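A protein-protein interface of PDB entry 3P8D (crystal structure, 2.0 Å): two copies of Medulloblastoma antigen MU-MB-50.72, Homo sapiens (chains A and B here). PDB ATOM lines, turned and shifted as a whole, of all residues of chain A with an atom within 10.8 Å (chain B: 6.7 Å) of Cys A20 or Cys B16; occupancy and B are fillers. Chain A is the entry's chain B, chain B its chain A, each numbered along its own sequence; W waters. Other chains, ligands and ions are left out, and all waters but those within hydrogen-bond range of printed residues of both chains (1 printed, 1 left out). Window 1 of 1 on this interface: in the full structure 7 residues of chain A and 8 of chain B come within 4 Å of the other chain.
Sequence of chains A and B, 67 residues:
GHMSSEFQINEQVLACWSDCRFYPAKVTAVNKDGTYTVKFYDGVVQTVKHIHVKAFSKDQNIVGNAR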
ATOM      1  N   LEU A  14      34.596  -3.734  31.168  1.00  0.00           N
ATOM      2  CA  LEU A  14      34.042  -2.616  30.425  1.00  0.00           C
ATOM      3  C   LEU A  14      32.573  -2.899  30.161  1.00  0.00           C
ATOM      4  O   LEU A  14      32.224  -3.943  29.616  1.00  0.00           O
ATOM      5  CB  LEU A  14      34.783  -2.415  29.104  1.00  0.00           C
ATOM      6  CG  LEU A  14      36.206  -1.871  29.210  1.00  0.00           C
ATOM      7  CD1 LEU A  14      36.881  -1.867  27.849  1.00  0.00           C
ATOM      8  CD2 LEU A  14      36.193  -0.476  29.810  1.00  0.00           C
ATOM      9  N   ALA A  15      31.714  -1.970  30.558  1.00  0.00           N
ATOM     10  CA  ALA A  15      30.279  -2.137  30.368  1.00  0.00           C
ATOM     11  C   ALA A  15      29.712  -0.976  29.559  1.00  0.00           C
ATOM     12  O   ALA A  15      30.188   0.153  29.663  1.00  0.00           O
ATOM     13  CB  ALA A  15      29.573  -2.263  31.706  1.00  0.00           C
ATOM     14  N   CYS A  16      28.694  -1.261  28.755  1.00  0.00           N
ATOM     15  CA  CYS A  16      28.087  -0.240  27.911  1.00  0.00           C
ATOM     16  C   CYS A  16      27.100   0.606  28.700  1.00  0.00           C
ATOM     17  O   CYS A  16      26.285   0.086  29.461  1.00  0.00           O
ATOM     18  CB  CYS A  16      27.386  -0.886  26.713  1.00  0.00           C
ATOM     19  SG  CYS A  16      26.645   0.285  25.559  1.00  0.00           S
ATOM     20  N   TRP A  17      27.178   1.918  28.524  1.00  0.00           N
ATOM     21  CA  TRP A  17      26.225   2.801  29.172  1.00  0.00           C
ATOM     22  C   TRP A  17      25.329   3.500  28.149  1.00  0.00           C
ATOM     23  O   TRP A  17      25.462   3.280  26.948  1.00  0.00           O
ATOM     24  CB  TRP A  17      26.926   3.804  30.088  1.00  0.00           C
ATOM     25  CG  TRP A  17      25.974   4.457  31.006  1.00  0.00           C
ATOM     26  CD1 TRP A  17      25.203   3.847  31.955  1.00  0.00           C
ATOM     27  CD2 TRP A  17      25.655   5.844  31.059  1.00  0.00           C
ATOM     28  NE1 TRP A  17      24.429   4.775  32.600  1.00  0.00           N
ATOM     29  CE2 TRP A  17      24.688   6.012  32.069  1.00  0.00           C
ATOM     30  CE3 TRP A  17      26.097   6.966  30.353  1.00  0.00           C
ATOM     31  CZ2 TRP A  17      24.156   7.256  32.392  1.00  0.00           C
ATOM     32  CZ3 TRP A  17      25.569   8.201  30.675  1.00  0.00           C
ATOM     33  CH2 TRP A  17      24.608   8.337  31.684  1.00  0.00           C
ATOM     34  N   SER A  18      24.415   4.333  28.637  1.00  0.00           N
ATOM     35  CA  SER A  18      23.357   4.912  27.810  1.00  0.00           C
ATOM     36  C   SER A  18      23.863   5.771  26.653  1.00  0.00           C
ATOM     37  O   SER A  18      23.159   5.955  25.657  1.00  0.00           O
ATOM     38  CB  SER A  18      22.402   5.733  28.676  1.00  0.00           C
ATOM     39  OG  SER A  18      21.926   4.967  29.761  1.00  0.00           O
ATOM     40  N   ASP A  19      25.073   6.307  26.781  1.00  0.00           N
ATOM     41  CA  ASP A  19      25.637   7.131  25.714  1.00  0.00           C
ATOM     42  C   ASP A  19      26.323   6.273  24.656  1.00  0.00           C
ATOM     43  O   ASP A  19      27.057   6.783  23.806  1.00  0.00           O
ATOM     44  CB  ASP A  19      26.616   8.157  26.282  1.00  0.00           C
ATOM     45  CG  ASP A  19      27.759   7.513  27.036  1.00  0.00           C
ATOM     46  OD1 ASP A  19      27.840   6.266  27.055  1.00  0.00           O
ATOM     47  OD2 ASP A  19      28.585   8.256  27.600  1.00  0.00           O
ATOM     48  N   CYS A  20      26.074   4.968  24.712  1.00  0.00           N
ATOM     49  CA  CYS A  20      26.678   4.021  23.785  1.00  0.00           C
ATOM     50  C   CYS A  20      28.205   4.080  23.824  1.00  0.00           C
ATOM     51  O   CYS A  20      28.867   3.947  22.798  1.00  0.00           O
ATOM     52  CB  CYS A  20      26.164   4.246  22.360  1.00  0.00           C
ATOM     53  SG  CYS A  20      25.339   2.813  21.626  1.00  0.00           S
ATOM     54  N   ARG A  21      28.752   4.280  25.018  1.00  0.00           N
ATOM     55  CA  ARG A  21      30.192   4.196  25.241  1.00  0.00           C
ATOM     56  C   ARG A  21      30.472   3.194  26.356  1.00  0.00           C
ATOM     57  O   ARG A  21      29.621   2.962  27.214  1.00  0.00           O
ATOM     58  CB  ARG A  21      30.763   5.563  25.630  1.00  0.00           C
ATOM     59  CG  ARG A  21      30.812   6.590  24.510  1.00  0.00           C
ATOM     60  CD  ARG A  21      31.284   7.944  25.037  1.00  0.00           C
ATOM     61  NE  ARG A  21      32.518   7.829  25.815  1.00  0.00           N
ATOM     62  CZ  ARG A  21      33.088   8.833  26.478  1.00  0.00           C
ATOM     63  NH1 ARG A  21      32.541  10.041  26.467  1.00  0.00           N
ATOM     64  NH2 ARG A  21      34.210   8.627  27.157  1.00  0.00           N
ATOM     65  N   PHE A  22      31.665   2.608  26.344  1.00  0.00           N
ATOM     66  CA  PHE A  22      32.055   1.656  27.376  1.00  0.00           C
ATOM     67  C   PHE A  22      32.777   2.344  28.527  1.00  0.00           C
ATOM     68  O   PHE A  22      33.602   3.230  28.317  1.00  0.00           O
ATOM     69  CB  PHE A  22      32.946   0.558  26.791  1.00  0.00           C
ATOM     70  CG  PHE A  22      32.199  -0.471  25.992  1.00  0.00           C
ATOM     71  CD1 PHE A  22      32.128  -0.382  24.609  1.00  0.00           C
ATOM     72  CD2 PHE A  22      31.567  -1.535  26.625  1.00  0.00           C
ATOM     73  CE1 PHE A  22      31.439  -1.336  23.871  1.00  0.00           C
ATOM     74  CE2 PHE A  22      30.877  -2.492  25.891  1.00  0.00           C
ATOM     75  CZ  PHE A  22      30.814  -2.392  24.516  1.00  0.00           C
ATOM     76  N   TYR A  23      32.459   1.928  29.747  1.00  0.00           N
ATOM     77  CA  TYR A  23      33.115   2.458  30.934  1.00  0.00           C
ATOM     78  C   TYR A  23      33.455   1.314  31.872  1.00  0.00           C
ATOM     79  O   TYR A  23      32.786   0.281  31.864  1.00  0.00           O
ATOM     80  CB  TYR A  23      32.216   3.462  31.659  1.00  0.00           C
ATOM     81  CG  TYR A  23      31.866   4.695  30.857  1.00  0.00           C
ATOM     82  CD1 TYR A  23      30.664   4.780  30.166  1.00  0.00           C
ATOM     83  CD2 TYR A  23      32.731   5.779  30.801  1.00  0.00           C
ATOM     84  CE1 TYR A  23      30.336   5.911  29.435  1.00  0.00           C
ATOM     85  CE2 TYR A  23      32.412   6.912  30.074  1.00  0.00           C
ATOM     86  CZ  TYR A  23      31.215   6.972  29.393  1.00  0.00           C
ATOM     87  OH  TYR A  23      30.899   8.098  28.671  1.00  0.00           O
ATOM     88  N   PHE A  40      29.137   1.051  37.939  1.00  0.00           N
ATOM     89  CA  PHE A  40      30.063   2.048  37.416  1.00  0.00           C
ATOM     90  C   PHE A  40      30.664   2.860  38.562  1.00  0.00           C
ATOM     91  O   PHE A  40      30.196   2.790  39.696  1.00  0.00           O
ATOM     92  CB  PHE A  40      29.360   2.982  36.430  1.00  0.00           C
ATOM     93  CG  PHE A  40      28.812   2.284  35.214  1.00  0.00           C
ATOM     94  CD1 PHE A  40      27.476   1.926  35.147  1.00  0.00           C
ATOM     95  CD2 PHE A  40      29.634   1.989  34.142  1.00  0.00           C
ATOM     96  CE1 PHE A  40      26.972   1.284  34.028  1.00  0.00           C
ATOM     97  CE2 PHE A  40      29.139   1.349  33.024  1.00  0.00           C
ATOM     98  CZ  PHE A  40      27.805   0.996  32.965  1.00  0.00           C
ATOM     99  N   GLN A  46      23.719  -1.665  36.882  1.00  0.00           N
ATOM    100  CA  GLN A  46      22.885  -2.254  35.844  1.00  0.00           C
ATOM    101  C   GLN A  46      23.177  -3.738  35.662  1.00  0.00           C
ATOM    102  O   GLN A  46      24.263  -4.219  35.984  1.00  0.00           O
ATOM    103  CB  GLN A  46      23.016  -1.496  34.515  1.00  0.00           C
ATOM    104  CG  GLN A  46      24.356  -1.641  33.819  1.00  0.00           C
ATOM    105  CD  GLN A  46      24.445  -0.817  32.543  1.00  0.00           C
ATOM    106  OE1 GLN A  46      23.771   0.204  32.397  1.00  0.00           O
ATOM    107  NE2 GLN A  46      25.277  -1.262  31.611  1.00  0.00           N
ATOM    108  N   HIS A  52      27.691  -8.763  26.511  1.00  0.00           N
ATOM    109  CA  HIS A  52      27.633  -7.313  26.352  1.00  0.00           C
ATOM    110  C   HIS A  52      28.697  -6.585  27.162  1.00  0.00           C
ATOM    111  O   HIS A  52      28.712  -5.357  27.223  1.00  0.00           O
ATOM    112  CB  HIS A  52      26.245  -6.779  26.714  1.00  0.00           C
ATOM    113  CG  HIS A  52      25.171  -7.207  25.762  1.00  0.00           C
ATOM    114  ND1 HIS A  52      25.444  -7.679  24.499  1.00  0.00           N
ATOM    115  CD2 HIS A  52      23.824  -7.233  25.897  1.00  0.00           C
ATOM    116  CE1 HIS A  52      24.307  -7.979  23.890  1.00  0.00           C
ATOM    117  NE2 HIS A  52      23.314  -7.719  24.715  1.00  0.00           N
ATOM    118  N   LYS A  54      33.123  -6.677  28.216  1.00  0.00           N
ATOM    119  CA  LYS A  54      34.408  -7.156  27.726  1.00  0.00           C
ATOM    120  C   LYS A  54      35.538  -6.824  28.683  1.00  0.00           C
ATOM    121  O   LYS A  54      35.373  -6.018  29.601  1.00  0.00           O
ATOM    122  CB  LYS A  54      34.695  -6.581  26.340  1.00  0.00           C
ATOM    123  CG  LYS A  54      34.621  -5.069  26.273  1.00  0.00           C
ATOM    124  CD  LYS A  54      34.793  -4.562  24.853  1.00  0.00           C
ATOM    125  CE  LYS A  54      34.836  -3.044  24.823  1.00  0.00           C
ATOM    126  NZ  LYS A  54      34.912  -2.509  23.438  1.00  0.00           N
ATOM    127  N   LEU B  14      18.259   6.949  15.548  1.00  0.00           N
ATOM    128  CA  LEU B  14      19.193   5.913  15.942  1.00  0.00           C
ATOM    129  C   LEU B  14      19.287   5.935  17.460  1.00  0.00           C
ATOM    130  O   LEU B  14      19.591   6.967  18.052  1.00  0.00           O
ATOM    131  CB  LEU B  14      20.568   6.141  15.315  1.00  0.00           C
ATOM    132  CG  LEU B  14      20.638   6.031  13.791  1.00  0.00           C
ATOM    133  CD1 LEU B  14      22.045   6.318  13.294  1.00  0.00           C
ATOM    134  CD2 LEU B  14      20.183   4.655  13.337  1.00  0.00           C
ATOM    135  N   ALA B  15      18.998   4.799  18.083  1.00  0.00           N
ATOM    136  CA  ALA B  15      19.053   4.691  19.536  1.00  0.00           C
ATOM    137  C   ALA B  15      20.066   3.626  19.944  1.00  0.00           C
ATOM    138  O   ALA B  15      20.303   2.673  19.203  1.00  0.00           O
ATOM    139  CB  ALA B  15      17.676   4.370  20.098  1.00  0.00           C
ATOM    140  N   CYS B  16      20.654   3.788  21.126  1.00  0.00           N
ATOM    141  CA  CYS B  16      21.658   2.847  21.614  1.00  0.00           C
ATOM    142  C   CYS B  16      21.005   1.632  22.262  1.00  0.00           C
ATOM    143  O   CYS B  16      20.056   1.762  23.040  1.00  0.00           O
ATOM    144  CB  CYS B  16      22.596   3.532  22.609  1.00  0.00           C
ATOM    145  SG  CYS B  16      24.004   2.529  23.130  1.00  0.00           S
ATOM    146  N   TRP B  17      21.503   0.449  21.925  1.00  0.00           N
ATOM    147  CA  TRP B  17      21.017  -0.765  22.561  1.00  0.00           C
ATOM    148  C   TRP B  17      22.108  -1.408  23.411  1.00  0.00           C
ATOM    149  O   TRP B  17      23.234  -0.912  23.462  1.00  0.00           O
ATOM    150  CB  TRP B  17      20.456  -1.749  21.534  1.00  0.00           C
ATOM    151  CG  TRP B  17      19.679  -2.839  22.184  1.00  0.00           C
ATOM    152  CD1 TRP B  17      18.543  -2.703  22.930  1.00  0.00           C
ATOM    153  CD2 TRP B  17      19.987  -4.233  22.172  1.00  0.00           C
ATOM    154  NE1 TRP B  17      18.122  -3.931  23.378  1.00  0.00           N
ATOM    155  CE2 TRP B  17      18.992  -4.888  22.925  1.00  0.00           C
ATOM    156  CE3 TRP B  17      21.008  -4.993  21.593  1.00  0.00           C
ATOM    157  CZ2 TRP B  17      18.989  -6.269  23.112  1.00  0.00           C
ATOM    158  CZ3 TRP B  17      21.002  -6.363  21.780  1.00  0.00           C
ATOM    159  CH2 TRP B  17      20.000  -6.987  22.532  1.00  0.00           C
ATOM    160  N   SER B  18      21.764  -2.507  24.073  1.00  0.00           N
ATOM    161  CA  SER B  18      22.627  -3.126  25.081  1.00  0.00           C
ATOM    162  C   SER B  18      23.981  -3.588  24.550  1.00  0.00           C
ATOM    163  O   SER B  18      24.936  -3.741  25.317  1.00  0.00           O
ATOM    164  CB  SER B  18      21.901  -4.305  25.731  1.00  0.00           C
ATOM    165  OG  SER B  18      20.581  -3.950  26.093  1.00  0.00           O
ATOM    166  N   ASP B  19      24.069  -3.821  23.244  1.00  0.00           N
ATOM    167  CA  ASP B  19      25.326  -4.263  22.646  1.00  0.00           C
ATOM    168  C   ASP B  19      26.212  -3.074  22.287  1.00  0.00           C
ATOM    169  O   ASP B  19      27.201  -3.218  21.569  1.00  0.00           O
ATOM    170  CB  ASP B  19      25.066  -5.125  21.411  1.00  0.00           C
ATOM    171  CG  ASP B  19      24.268  -4.397  20.350  1.00  0.00           C
ATOM    172  OD1 ASP B  19      23.978  -5.015  19.308  1.00  0.00           O
ATOM    173  OD2 ASP B  19      23.926  -3.214  20.561  1.00  0.00           O
ATOM    174  N   CYS B  20      25.849  -1.905  22.807  1.00  0.00           N
ATOM    175  CA  CYS B  20      26.560  -0.662  22.534  1.00  0.00           C
ATOM    176  C   CYS B  20      26.640  -0.375  21.039  1.00  0.00           C
ATOM    177  O   CYS B  20      27.665   0.085  20.541  1.00  0.00           O
ATOM    178  CB  CYS B  20      27.958  -0.667  23.160  1.00  0.00           C
ATOM    179  SG  CYS B  20      28.249   0.646  24.374  1.00  0.00           S
ATOM    180  N   ARG B  21      25.551  -0.654  20.332  1.00  0.00           N
ATOM    181  CA  ARG B  21      25.417  -0.270  18.930  1.00  0.00           C
ATOM    182  C   ARG B  21      24.112   0.486  18.739  1.00  0.00           C
ATOM    183  O   ARG B  21      23.169   0.319  19.512  1.00  0.00           O
ATOM    184  CB  ARG B  21      25.435  -1.500  18.020  1.00  0.00           C
ATOM    185  CG  ARG B  21      26.774  -2.206  17.947  1.00  0.00           C
ATOM    186  CD  ARG B  21      26.668  -3.472  17.114  1.00  0.00           C
ATOM    187  NE  ARG B  21      27.970  -4.083  16.865  1.00  0.00           N
ATOM    188  CZ  ARG B  21      28.562  -4.950  17.682  1.00  0.00           C
ATOM    189  NH1 ARG B  21      27.971  -5.310  18.813  1.00  0.00           N
ATOM    190  NH2 ARG B  21      29.747  -5.455  17.368  1.00  0.00           N
ATOM    191  N   PHE B  22      24.066   1.319  17.706  1.00  0.00           N
ATOM    192  CA  PHE B  22      22.867   2.077  17.390  1.00  0.00           C
ATOM    193  C   PHE B  22      21.983   1.324  16.405  1.00  0.00           C
ATOM    194  O   PHE B  22      22.472   0.705  15.460  1.00  0.00           O
ATOM    195  CB  PHE B  22      23.241   3.447  16.819  1.00  0.00           C
ATOM    196  CG  PHE B  22      23.760   4.415  17.844  1.00  0.00           C
ATOM    197  CD1 PHE B  22      25.118   4.501  18.118  1.00  0.00           C
ATOM    198  CD2 PHE B  22      22.888   5.245  18.535  1.00  0.00           C
ATOM    199  CE1 PHE B  22      25.597   5.398  19.062  1.00  0.00           C
ATOM    200  CE2 PHE B  22      23.361   6.144  19.481  1.00  0.00           C
ATOM    201  CZ  PHE B  22      24.716   6.220  19.744  1.00  0.00           C
ATOM    202  N   TYR B  23      20.677   1.371  16.638  1.00  0.00           N
ATOM    203  CA  TYR B  23      19.712   0.782  15.721  1.00  0.00           C
ATOM    204  C   TYR B  23      18.561   1.750  15.520  1.00  0.00           C
ATOM    205  O   TYR B  23      18.279   2.571  16.390  1.00  0.00           O
ATOM    206  CB  TYR B  23      19.169  -0.543  16.262  1.00  0.00           C
ATOM    207  CG  TYR B  23      20.209  -1.617  16.459  1.00  0.00           C
ATOM    208  CD1 TYR B  23      20.794  -1.825  17.702  1.00  0.00           C
ATOM    209  CD2 TYR B  23      20.602  -2.434  15.405  1.00  0.00           C
ATOM    210  CE1 TYR B  23      21.746  -2.812  17.889  1.00  0.00           C
ATOM    211  CE2 TYR B  23      21.552  -3.423  15.585  1.00  0.00           C
ATOM    212  CZ  TYR B  23      22.121  -3.607  16.828  1.00  0.00           C
ATOM    213  OH  TYR B  23      23.067  -4.589  17.008  1.00  0.00           O
ATOM    214  N   PHE B  40      12.314  -0.232  19.038  1.00  0.00           N
ATOM    215  CA  PHE B  40      13.111  -0.841  17.978  1.00  0.00           C
ATOM    216  C   PHE B  40      12.228  -1.687  17.062  1.00  0.00           C
ATOM    217  O   PHE B  40      11.060  -1.924  17.363  1.00  0.00           O
ATOM    218  CB  PHE B  40      14.234  -1.695  18.565  1.00  0.00           C
ATOM    219  CG  PHE B  40      15.231  -0.913  19.377  1.00  0.00           C
ATOM    220  CD1 PHE B  40      15.160  -0.900  20.759  1.00  0.00           C
ATOM    221  CD2 PHE B  40      16.235  -0.190  18.756  1.00  0.00           C
ATOM    222  CE1 PHE B  40      16.079  -0.181  21.511  1.00  0.00           C
ATOM    223  CE2 PHE B  40      17.155   0.531  19.496  1.00  0.00           C
ATOM    224  CZ  PHE B  40      17.077   0.536  20.881  1.00  0.00           C
ATOM    225  N   GLN B  46      12.339   1.275  24.994  1.00  0.00           N
ATOM    226  CA  GLN B  46      13.153   1.857  26.052  1.00  0.00           C
ATOM    227  C   GLN B  46      13.007   3.374  26.108  1.00  0.00           C
ATOM    228  O   GLN B  46      12.673   4.017  25.113  1.00  0.00           O
ATOM    229  CB  GLN B  46      14.627   1.446  25.926  1.00  0.00           C
ATOM    230  CG  GLN B  46      15.342   1.956  24.692  1.00  0.00           C
ATOM    231  CD  GLN B  46      16.805   1.539  24.658  1.00  0.00           C
ATOM    232  OE1 GLN B  46      17.164   0.438  25.079  1.00  0.00           O
ATOM    233  NE2 GLN B  46      17.656   2.423  24.159  1.00  0.00           N
ATOM    234  N   VAL B  48      14.911   6.903  26.665  1.00  0.00           N
ATOM    235  CA  VAL B  48      16.266   7.439  26.575  1.00  0.00           C
ATOM    236  C   VAL B  48      16.268   8.960  26.585  1.00  0.00           C
ATOM    237  O   VAL B  48      15.288   9.594  26.178  1.00  0.00           O
ATOM    238  CB  VAL B  48      16.984   6.939  25.307  1.00  0.00           C
ATOM    239  CG1 VAL B  48      17.075   5.425  25.311  1.00  0.00           C
ATOM    240  CG2 VAL B  48      16.252   7.420  24.064  1.00  0.00           C
ATOM    241  N   HIS B  52      21.018  11.133  23.866  1.00  0.00           N
ATOM    242  CA  HIS B  52      21.511   9.780  23.635  1.00  0.00           C
ATOM    243  C   HIS B  52      20.942   9.150  22.368  1.00  0.00           C
ATOM    244  O   HIS B  52      21.152   7.966  22.101  1.00  0.00           O
ATOM    245  CB  HIS B  52      21.242   8.893  24.852  1.00  0.00           C
ATOM    246  CG  HIS B  52      22.055   9.265  26.049  1.00  0.00           C
ATOM    247  ND1 HIS B  52      21.627   9.039  27.343  1.00  0.00           N
ATOM    248  CD2 HIS B  52      23.273   9.846  26.156  1.00  0.00           C
ATOM    249  CE1 HIS B  52      22.545   9.467  28.187  1.00  0.00           C
ATOM    250  NE2 HIS B  52      23.557   9.962  27.492  1.00  0.00           N
ATOM    251  N   VAL B  53      20.221   9.946  21.590  1.00  0.00           N
ATOM    252  CA  VAL B  53      19.773   9.507  20.275  1.00  0.00           C
ATOM    253  C   VAL B  53      20.284  10.483  19.227  1.00  0.00           C
ATOM    254  O   VAL B  53      20.671  11.608  19.546  1.00  0.00           O
ATOM    255  CB  VAL B  53      18.242   9.409  20.183  1.00  0.00           C
ATOM    256  CG1 VAL B  53      17.705   8.480  21.257  1.00  0.00           C
ATOM    257  CG2 VAL B  53      17.613  10.787  20.298  1.00  0.00           C
HETATM  258  O   HOH W   1      27.654  -3.807  25.101  1.00  0.00           O
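The side-chain sulfur of Cys B16 is disulfide-bonded to the side-chain sulfur of Cys A20 (2.0 Å). SG of Cys A16 is disulfide-bonded to SG of Cys B20, 2.0 Å away. N of Arg A21 sits at hydrogen-bond distance from SG of Cys B20 (3.7 Å). N of Arg B21 sits at hydrogen-bond distance from SG of Cys A20, at 3.7 Å. The backbone carbonyl oxygen (O) of Cys A20 lies close to the side-chain sulfur (SG) of Cys B20, at 3.7 Å.
Printed residues of chain B that touch a printed residue of chain A: Cys B16, Trp B17, Ser B18, Asp B19, Cys B20, Arg B21, Phe B22 and His B52. Hydrophobic or aromatic side chains of chain B within 4 Å of the printed part of chain A: Trp B17, Phe B22 and His B52. Of the 14 printed residues of chain A, 7 touch a printed residue of chain B. Among the printed residues, 13 pairs touch across the chains. Among the printed residues, no Asp or Glu carboxylate lies within 4 Å of a Lys or Arg side-chain nitrogen of the other chain.
Of chain B, only Cys B16 (2.0 Å), Cys B20 (3.5 Å), Arg B21 (3.7 Å) and Phe B22 (3.5 Å) come within 4 Å of Cys A20. Printed residues of chain A within 4 Å of Cys B16: Ser A18 (3.9 Å) and Cys A20 (2.0 Å). Ala B15 touches none of the printed residues of chain A. Phe B22 touches just one residue of chain A: Cys A20. Of the printed residues of chain B, Phe A22 touches Cys B20 (3.6 Å). Printed residues of chain B within 4 Å of His A52: Trp B17, Ser B18 and Asp B19. Printed residues of chain B within 4 Å of Ser A18: Cys B16 (3.9 Å) and His B52 (3.5 Å). The nearest residue of chain B that does not touch Cys A20 is Trp B17 (4.5 Å). The nearest residue of chain A that does not touch Cys B16 is Trp A17 (4.2 Å).
Cys A16 touches Cys B20, and with the chains exchanged Cys A20 touches Cys B16. Ser A18 touches Cys B16, but with the chains exchanged Cys A16 does not touch Ser B18 (4.01 Å). Asp A19 touches His B52, and with the chains exchanged His A52 touches Asp B19. Cys A20 touches Arg B21, and with the chains exchanged Arg A21 touches Cys B20. 13 positions are printed for both chains.
O of Cys B16 lies within hydrogen-bond range of NE2 of Gln B46 (2.7 Å). The backbone NH (N) of Arg B21 lies within hydrogen-bond range of the side-chain carboxylate (OD2) of Asp B19 (3.0 Å). OH of Tyr B23 sits at hydrogen-bond distance from OD1 of Asp B19, 2.5 Å away. The backbone carbonyl oxygen of Cys A16 lies within hydrogen-bond range of the side-chain amide nitrogen of Gln A46, at 2.7 Å. OH of Tyr A23 sits at hydrogen-bond distance from OD2 of Asp A19 (2.6 Å). The guanidinium group (NE) of Arg A21 lies close to the side-chain hydroxyl (OH) of Tyr A23 (3.3 Å).
Water W1 lies within hydrogen-bond range of the backbone carbonyl oxygen of Ser B18 (2.7 Å), the backbone carbonyl oxygen of His A52 (2.8 Å) and the backbone NH of Cys B20 (3.5 Å).
Among the printed residues, pairs that only touch across the chains: His A52 with Ser B18 (3.5 Å), Ser A18 with His B52 (3.5 Å), Cys A20 with Phe B22 (3.5 Å), Phe A22 with Cys B20 (3.6 Å), Asp A19 with His B52 (3.6 Å), His A52 with Asp B19 (3.9 Å), Ser A18 with Cys B16 (3.9 Å) and His A52 with Trp B17 (3.97 Å).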
